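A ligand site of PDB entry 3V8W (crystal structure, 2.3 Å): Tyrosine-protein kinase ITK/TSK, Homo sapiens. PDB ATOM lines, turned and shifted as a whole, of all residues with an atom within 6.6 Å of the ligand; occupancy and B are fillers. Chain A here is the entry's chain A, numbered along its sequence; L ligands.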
ATOM      1  N   ILE A  15      17.809  16.937   3.940  1.00  0.00           N
ATOM      2  CA  ILE A  15      17.748  15.829   2.984  1.00  0.00           C
ATOM      3  C   ILE A  15      18.998  14.931   2.923  1.00  0.00           C
ATOM      4  O   ILE A  15      18.926  13.815   2.407  1.00  0.00           O
ATOM      5  CB  ILE A  15      17.268  16.296   1.573  1.00  0.00           C
ATOM      6  CG1 ILE A  15      18.134  17.476   1.038  1.00  0.00           C
ATOM      7  CG2 ILE A  15      15.765  16.630   1.589  1.00  0.00           C
ATOM      8  CD1 ILE A  15      17.996  17.803  -0.460  1.00  0.00           C
ATOM      9  N   GLY A  16      20.113  15.426   3.463  1.00  0.00           N
ATOM     10  CA  GLY A  16      21.378  14.710   3.486  1.00  0.00           C
ATOM     11  C   GLY A  16      22.252  15.027   4.681  1.00  0.00           C
ATOM     12  O   GLY A  16      22.068  16.055   5.335  1.00  0.00           O
ATOM     13  N   VAL A  23      23.039  18.491   4.096  1.00  0.00           N
ATOM     14  CA  VAL A  23      22.407  18.898   2.840  1.00  0.00           C
ATOM     15  C   VAL A  23      20.932  19.202   3.125  1.00  0.00           C
ATOM     16  O   VAL A  23      20.211  18.345   3.632  1.00  0.00           O
ATOM     17  CB  VAL A  23      22.576  17.861   1.686  1.00  0.00           C
ATOM     18  CG1 VAL A  23      21.957  18.367   0.391  1.00  0.00           C
ATOM     19  CG2 VAL A  23      24.038  17.493   1.480  1.00  0.00           C
ATOM     20  N   LEU A  25      17.139  20.927   1.633  1.00  0.00           N
ATOM     21  CA  LEU A  25      16.288  21.313   0.515  1.00  0.00           C
ATOM     22  C   LEU A  25      15.777  22.700   0.859  1.00  0.00           C
ATOM     23  O   LEU A  25      15.314  22.930   1.984  1.00  0.00           O
ATOM     24  CB  LEU A  25      15.110  20.312   0.345  1.00  0.00           C
ATOM     25  CG  LEU A  25      13.877  20.782  -0.466  1.00  0.00           C
ATOM     26  CD1 LEU A  25      14.196  20.951  -1.946  1.00  0.00           C
ATOM     27  CD2 LEU A  25      12.726  19.821  -0.305  1.00  0.00           C
ATOM     28  N   VAL A  34      16.527  24.740  -4.444  1.00  0.00           N
ATOM     29  CA  VAL A  34      17.983  24.623  -4.274  1.00  0.00           C
ATOM     30  C   VAL A  34      18.390  23.594  -3.214  1.00  0.00           C
ATOM     31  O   VAL A  34      17.625  23.321  -2.290  1.00  0.00           O
ATOM     32  CB  VAL A  34      18.685  25.990  -4.057  1.00  0.00           C
ATOM     33  CG1 VAL A  34      18.655  26.862  -5.315  1.00  0.00           C
ATOM     34  CG2 VAL A  34      18.128  26.746  -2.855  1.00  0.00           C
ATOM     35  N   ALA A  35      19.598  23.033  -3.365  1.00  0.00           N
ATOM     36  CA  ALA A  35      20.193  22.101  -2.410  1.00  0.00           C
ATOM     37  C   ALA A  35      21.329  22.854  -1.715  1.00  0.00           C
ATOM     38  O   ALA A  35      22.290  23.274  -2.372  1.00  0.00           O
ATOM     39  CB  ALA A  35      20.717  20.869  -3.122  1.00  0.00           C
ATOM     40  N   ILE A  36      21.174  23.080  -0.402  1.00  0.00           N
ATOM     41  CA  ILE A  36      22.123  23.836   0.421  1.00  0.00           C
ATOM     42  C   ILE A  36      23.061  22.909   1.203  1.00  0.00           C
ATOM     43  O   ILE A  36      22.609  22.170   2.093  1.00  0.00           O
ATOM     44  CB  ILE A  36      21.354  24.849   1.327  1.00  0.00           C
ATOM     45  CG1 ILE A  36      20.378  25.725   0.506  1.00  0.00           C
ATOM     46  CG2 ILE A  36      22.318  25.718   2.122  1.00  0.00           C
ATOM     47  CD1 ILE A  36      19.054  26.056   1.226  1.00  0.00           C
ATOM     48  N   LYS A  37      24.370  22.958   0.883  1.00  0.00           N
ATOM     49  CA  LYS A  37      25.415  22.168   1.533  1.00  0.00           C
ATOM     50  C   LYS A  37      26.133  23.038   2.588  1.00  0.00           C
ATOM     51  O   LYS A  37      26.959  23.878   2.237  1.00  0.00           O
ATOM     52  CB  LYS A  37      26.398  21.599   0.480  1.00  0.00           C
ATOM     53  CG  LYS A  37      27.615  20.844   1.024  1.00  0.00           C
ATOM     54  CD  LYS A  37      27.295  19.436   1.522  1.00  0.00           C
ATOM     55  CE  LYS A  37      28.499  18.768   2.140  1.00  0.00           C
ATOM     56  N   MET A  56      34.344  24.428  -9.518  1.00  0.00           N
ATOM     57  CA  MET A  56      33.062  23.891  -9.982  1.00  0.00           C
ATOM     58  C   MET A  56      32.240  24.895 -10.806  1.00  0.00           C
ATOM     59  O   MET A  56      31.509  24.495 -11.709  1.00  0.00           O
ATOM     60  CB  MET A  56      32.231  23.329  -8.823  1.00  0.00           C
ATOM     61  CG  MET A  56      32.733  21.977  -8.326  1.00  0.00           C
ATOM     62  SD  MET A  56      31.541  21.076  -7.311  1.00  0.00           S
ATOM     63  CE  MET A  56      31.860  21.793  -5.714  1.00  0.00           C
ATOM     64  N   VAL A  65      27.167  18.846 -12.012  1.00  0.00           N
ATOM     65  CA  VAL A  65      26.271  19.628 -11.137  1.00  0.00           C
ATOM     66  C   VAL A  65      26.694  21.097 -11.127  1.00  0.00           C
ATOM     67  O   VAL A  65      27.879  21.404 -11.005  1.00  0.00           O
ATOM     68  CB  VAL A  65      26.140  19.026  -9.705  1.00  0.00           C
ATOM     69  CG1 VAL A  65      25.020  19.720  -8.924  1.00  0.00           C
ATOM     70  CG2 VAL A  65      25.898  17.533  -9.753  1.00  0.00           C
ATOM     71  N   LEU A  79      27.120  26.226   0.407  1.00  0.00           N
ATOM     72  CA  LEU A  79      27.128  26.211  -1.055  1.00  0.00           C
ATOM     73  C   LEU A  79      25.697  26.053  -1.564  1.00  0.00           C
ATOM     74  O   LEU A  79      24.950  25.213  -1.046  1.00  0.00           O
ATOM     75  CB  LEU A  79      27.999  25.055  -1.608  1.00  0.00           C
ATOM     76  CG  LEU A  79      29.395  24.845  -1.027  1.00  0.00           C
ATOM     77  CD1 LEU A  79      29.997  23.533  -1.504  1.00  0.00           C
ATOM     78  CD2 LEU A  79      30.335  25.982  -1.345  1.00  0.00           C
ATOM     79  N   PHE A  81      23.610  24.791  -4.458  1.00  0.00           N
ATOM     80  CA  PHE A  81      23.572  23.912  -5.629  1.00  0.00           C
ATOM     81  C   PHE A  81      22.185  23.843  -6.248  1.00  0.00           C
ATOM     82  O   PHE A  81      21.193  24.163  -5.581  1.00  0.00           O
ATOM     83  CB  PHE A  81      24.009  22.492  -5.241  1.00  0.00           C
ATOM     84  CG  PHE A  81      25.485  22.265  -5.084  1.00  0.00           C
ATOM     85  CD1 PHE A  81      26.078  22.292  -3.825  1.00  0.00           C
ATOM     86  CD2 PHE A  81      26.281  21.959  -6.184  1.00  0.00           C
ATOM     87  CE1 PHE A  81      27.443  22.045  -3.674  1.00  0.00           C
ATOM     88  CE2 PHE A  81      27.647  21.712  -6.033  1.00  0.00           C
ATOM     89  CZ  PHE A  81      28.229  21.769  -4.783  1.00  0.00           C
ATOM     90  N   GLU A  82      22.103  23.386  -7.508  1.00  0.00           N
ATOM     91  CA  GLU A  82      20.827  23.166  -8.204  1.00  0.00           C
ATOM     92  C   GLU A  82      20.188  21.903  -7.610  1.00  0.00           C
ATOM     93  O   GLU A  82      20.914  20.964  -7.252  1.00  0.00           O
ATOM     94  CB  GLU A  82      21.022  23.033  -9.737  1.00  0.00           C
ATOM     95  CG  GLU A  82      21.953  21.916 -10.191  1.00  0.00           C
ATOM     96  CD  GLU A  82      21.970  21.571 -11.672  1.00  0.00           C
ATOM     97  OE1 GLU A  82      21.092  22.053 -12.417  1.00  0.00           O
ATOM     98  OE2 GLU A  82      22.864  20.788 -12.077  1.00  0.00           O
ATOM     99  N   PHE A  83      18.857  21.896  -7.439  1.00  0.00           N
ATOM    100  CA  PHE A  83      18.189  20.736  -6.861  1.00  0.00           C
ATOM    101  C   PHE A  83      17.994  19.605  -7.863  1.00  0.00           C
ATOM    102  O   PHE A  83      17.398  19.803  -8.926  1.00  0.00           O
ATOM    103  CB  PHE A  83      16.881  21.130  -6.150  1.00  0.00           C
ATOM    104  CG  PHE A  83      16.181  19.966  -5.471  1.00  0.00           C
ATOM    105  CD1 PHE A  83      16.701  19.405  -4.314  1.00  0.00           C
ATOM    106  CD2 PHE A  83      15.012  19.442  -5.990  1.00  0.00           C
ATOM    107  CE1 PHE A  83      16.068  18.333  -3.686  1.00  0.00           C
ATOM    108  CE2 PHE A  83      14.366  18.372  -5.360  1.00  0.00           C
ATOM    109  CZ  PHE A  83      14.902  17.823  -4.214  1.00  0.00           C
ATOM    110  N   MET A  84      18.490  18.406  -7.512  1.00  0.00           N
ATOM    111  CA  MET A  84      18.349  17.191  -8.307  1.00  0.00           C
ATOM    112  C   MET A  84      17.223  16.375  -7.683  1.00  0.00           C
ATOM    113  O   MET A  84      17.330  15.930  -6.548  1.00  0.00           O
ATOM    114  CB  MET A  84      19.679  16.403  -8.359  1.00  0.00           C
ATOM    115  CG  MET A  84      20.834  17.180  -8.985  1.00  0.00           C
ATOM    116  SD  MET A  84      20.681  17.486 -10.763  1.00  0.00           S
ATOM    117  CE  MET A  84      21.225  15.914 -11.404  1.00  0.00           C
ATOM    118  N   GLU A  85      16.096  16.257  -8.424  1.00  0.00           N
ATOM    119  CA  GLU A  85      14.841  15.606  -8.031  1.00  0.00           C
ATOM    120  C   GLU A  85      14.957  14.240  -7.338  1.00  0.00           C
ATOM    121  O   GLU A  85      14.290  14.022  -6.327  1.00  0.00           O
ATOM    122  CB  GLU A  85      13.859  15.533  -9.216  1.00  0.00           C
ATOM    123  CG  GLU A  85      13.237  16.864  -9.599  1.00  0.00           C
ATOM    124  CD  GLU A  85      12.174  17.404  -8.663  1.00  0.00           C
ATOM    125  OE1 GLU A  85      11.163  16.708  -8.431  1.00  0.00           O
ATOM    126  OE2 GLU A  85      12.328  18.559  -8.200  1.00  0.00           O
ATOM    127  N   HIS A  86      15.769  13.328  -7.893  1.00  0.00           N
ATOM    128  CA  HIS A  86      15.906  11.963  -7.372  1.00  0.00           C
ATOM    129  C   HIS A  86      17.103  11.710  -6.444  1.00  0.00           C
ATOM    130  O   HIS A  86      17.242  10.608  -5.896  1.00  0.00           O
ATOM    131  CB  HIS A  86      15.776  10.924  -8.494  1.00  0.00           C
ATOM    132  CG  HIS A  86      14.482  11.044  -9.232  1.00  0.00           C
ATOM    133  ND1 HIS A  86      13.319  10.457  -8.751  1.00  0.00           N
ATOM    134  CD2 HIS A  86      14.198  11.707 -10.376  1.00  0.00           C
ATOM    135  CE1 HIS A  86      12.376  10.772  -9.627  1.00  0.00           C
ATOM    136  NE2 HIS A  86      12.854  11.524 -10.618  1.00  0.00           N
ATOM    137  N   GLY A  87      17.922  12.740  -6.240  1.00  0.00           N
ATOM    138  CA  GLY A  87      19.079  12.723  -5.354  1.00  0.00           C
ATOM    139  C   GLY A  87      20.194  11.764  -5.702  1.00  0.00           C
ATOM    140  O   GLY A  87      20.459  11.513  -6.879  1.00  0.00           O
ATOM    141  N   CYS A  88      20.858  11.242  -4.659  1.00  0.00           N
ATOM    142  CA  CYS A  88      21.991  10.317  -4.696  1.00  0.00           C
ATOM    143  C   CYS A  88      21.743   9.076  -5.558  1.00  0.00           C
ATOM    144  O   CYS A  88      20.714   8.419  -5.395  1.00  0.00           O
ATOM    145  CB  CYS A  88      22.413   9.944  -3.270  1.00  0.00           C
ATOM    146  SG  CYS A  88      23.841   8.846  -3.173  1.00  0.00           S
ATOM    147  N   ASN A 133      28.583  10.034  -4.889  1.00  0.00           N
ATOM    148  CA  ASN A 133      28.953  11.377  -5.350  1.00  0.00           C
ATOM    149  C   ASN A 133      28.323  11.729  -6.719  1.00  0.00           C
ATOM    150  O   ASN A 133      28.707  12.715  -7.340  1.00  0.00           O
ATOM    151  CB  ASN A 133      30.475  11.532  -5.365  1.00  0.00           C
ATOM    152  CG  ASN A 133      31.123  11.406  -4.002  1.00  0.00           C
ATOM    153  OD1 ASN A 133      30.865  12.190  -3.082  1.00  0.00           O
ATOM    154  ND2 ASN A 133      31.989  10.409  -3.851  1.00  0.00           N
ATOM    155  N   LEU A 135      24.528  12.359  -8.818  1.00  0.00           N
ATOM    156  CA  LEU A 135      23.141  12.744  -8.594  1.00  0.00           C
ATOM    157  C   LEU A 135      22.220  12.455  -9.777  1.00  0.00           C
ATOM    158  O   LEU A 135      22.652  12.516 -10.924  1.00  0.00           O
ATOM    159  CB  LEU A 135      23.045  14.214  -8.164  1.00  0.00           C
ATOM    160  CG  LEU A 135      23.636  14.546  -6.787  1.00  0.00           C
ATOM    161  CD1 LEU A 135      24.239  15.925  -6.776  1.00  0.00           C
ATOM    162  CD2 LEU A 135      22.610  14.392  -5.690  1.00  0.00           C
ATOM    163  N   VAL A 136      20.948  12.159  -9.475  1.00  0.00           N
ATOM    164  CA  VAL A 136      19.902  11.826 -10.444  1.00  0.00           C
ATOM    165  C   VAL A 136      18.898  12.992 -10.526  1.00  0.00           C
ATOM    166  O   VAL A 136      18.349  13.400  -9.503  1.00  0.00           O
ATOM    167  CB  VAL A 136      19.190  10.485 -10.119  1.00  0.00           C
ATOM    168  CG1 VAL A 136      18.297  10.027 -11.277  1.00  0.00           C
ATOM    169  CG2 VAL A 136      20.173   9.388  -9.744  1.00  0.00           C
ATOM    170  N   SER A 145      29.114  15.071  -9.139  1.00  0.00           N
ATOM    171  CA  SER A 145      29.270  16.056  -8.069  1.00  0.00           C
ATOM    172  C   SER A 145      30.587  15.840  -7.314  1.00  0.00           C
ATOM    173  O   SER A 145      31.248  14.822  -7.536  1.00  0.00           O
ATOM    174  CB  SER A 145      28.085  15.977  -7.104  1.00  0.00           C
ATOM    175  OG  SER A 145      28.010  17.129  -6.291  1.00  0.00           O
ATOM    176  N   ASP A 146      30.960  16.799  -6.424  1.00  0.00           N
ATOM    177  CA  ASP A 146      32.187  16.787  -5.601  1.00  0.00           C
ATOM    178  C   ASP A 146      33.480  16.726  -6.434  1.00  0.00           C
ATOM    179  O   ASP A 146      34.485  16.168  -5.986  1.00  0.00           O
ATOM    180  CB  ASP A 146      32.135  15.687  -4.515  1.00  0.00           C
ATOM    181  CG  ASP A 146      31.886  16.188  -3.102  1.00  0.00           C
ATOM    182  OD1 ASP A 146      31.111  15.541  -2.367  1.00  0.00           O
ATOM    183  OD2 ASP A 146      32.510  17.199  -2.720  1.00  0.00           O
HETATM  184  C1  LIG L   1      13.648  11.427  -3.364  1.00  0.00           C
HETATM  185  C2  LIG L   1      14.984  12.180  -3.367  1.00  0.00           C
HETATM  186  C3  LIG L   1      15.065  13.233  -2.252  1.00  0.00           C
HETATM  187  C4  LIG L   1      13.993  14.319  -2.504  1.00  0.00           C
HETATM  188  C5  LIG L   1      13.996  15.375  -1.397  1.00  0.00           C
HETATM  189  O1  LIG L   1      14.801  12.603  -0.997  1.00  0.00           O
HETATM  190  C6  LIG L   1      16.469  13.862  -2.271  1.00  0.00           C
HETATM  191  C7  LIG L   1      16.821  14.782  -3.273  1.00  0.00           C
HETATM  192  C8  LIG L   1      17.417  13.509  -1.306  1.00  0.00           C
HETATM  193  C9  LIG L   1      18.691  14.078  -1.321  1.00  0.00           C
HETATM  194  C10 LIG L   1      19.027  14.986  -2.322  1.00  0.00           C
HETATM  195  C11 LIG L   1      20.143  15.675  -2.579  1.00  0.00           C
HETATM  196  C12 LIG L   1      18.094  15.351  -3.278  1.00  0.00           C
HETATM  197  N1  LIG L   1      18.690  16.218  -4.090  1.00  0.00           N
HETATM  198  C13 LIG L   1      19.932  16.426  -3.653  1.00  0.00           C
HETATM  199  C14 LIG L   1      20.849  17.286  -4.258  1.00  0.00           C
HETATM  200  N2  LIG L   1      20.661  18.125  -5.271  1.00  0.00           N
HETATM  201  N3  LIG L   1      21.714  18.731  -5.537  1.00  0.00           N
HETATM  202  C15 LIG L   1      22.713  18.373  -4.723  1.00  0.00           C
HETATM  203  C16 LIG L   1      24.019  18.640  -4.477  1.00  0.00           C
HETATM  204  C17 LIG L   1      22.171  17.419  -3.875  1.00  0.00           C
HETATM  205  S1  LIG L   1      23.389  16.926  -2.834  1.00  0.00           S
HETATM  206  C18 LIG L   1      24.577  17.941  -3.475  1.00  0.00           C
HETATM  207  C19 LIG L   1      25.900  17.958  -3.015  1.00  0.00           C
HETATM  208  C20 LIG L   1      26.895  18.596  -3.759  1.00  0.00           C
HETATM  209  C21 LIG L   1      28.209  18.608  -3.319  1.00  0.00           C
HETATM  210  C22 LIG L   1      28.549  17.972  -2.127  1.00  0.00           C
HETATM  211  C23 LIG L   1      27.566  17.318  -1.374  1.00  0.00           C
HETATM  212  C24 LIG L   1      26.246  17.315  -1.824  1.00  0.00           C
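N of Met 84 sits close to N2 of the ligand (3.1 Å). The backbone carbonyl oxygen (O) of Met 84 sits at hydrogen-bond distance from a nitrogen (N1) of the ligand (2.8 Å). A nitrogen (N2) of the ligand sits at hydrogen-bond distance from the backbone carbonyl oxygen (O) of Glu 82.
The backbone carbonyl oxygen (O) of Asn 133 is in hydrogen-bond range of the backbone NH (N) of Ser 145, at 3.0 Å. The backbone carbonyl oxygen of Ala 35 is in hydrogen-bond range of the backbone NH of Phe 81. O of Gly 87 is in hydrogen-bond range of N of Val 136, 2.7 Å away. The backbone NH of Ile 15 sits at hydrogen-bond distance from the backbone carbonyl oxygen of Val 23. The side-chain amide oxygen (OD1) of Asn 133 lies close to the side-chain carboxylate (OD1) of Asp 146, 3.4 Å away. The backbone NH (N) of Leu 79 is in hydrogen-bond range of the backbone carbonyl oxygen (O) of Lys 37, at 3.0 Å. O of Val 136 lies within hydrogen-bond range of N of His 86, 3.0 Å away. The backbone NH (N) of Val 23 lies within hydrogen-bond range of the backbone carbonyl oxygen (O) of Gly 16 (2.9 Å).
Ile 15 touches the ligand (CD1 to C10, 3.5 Å). Val 23 touches the ligand (CG1 to S1, 3.8 Å). Ala 35 touches the ligand (CB to N3, 3.4 Å). Lys 37 touches the ligand. CZ of Phe 81 touches C21 of the ligand, at 3.5 Å. Phe 83 touches the ligand (CE1 to N1, 3.4 Å). Glu 85 touches the ligand (O to C2, 3.6 Å). His 86 touches the ligand. Gly 87 touches the ligand. Leu 135 touches the ligand (CD1 to C15, 3.5 Å). OG of Ser 145 touches C20 of the ligand (3.1 Å). Asp 146 touches the ligand (OD1 to C22, 3.5 Å). Hydrophobic or aromatic side chains within 4 Å of the ligand: Ile 15, Val 23, Ala 35, Phe 81, Phe 83, Met 84 and Leu 135. Within 4 Å of the ligand: Ile 15, Val 23, Ala 35, Lys 37, Phe 81, Glu 82, Phe 83, Met 84, Glu 85, His 86, Gly 87, Leu 135, Ser 145 and Asp 146. The nearest printed residue that does not touch the ligand is Val 65 (4.7 Å).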
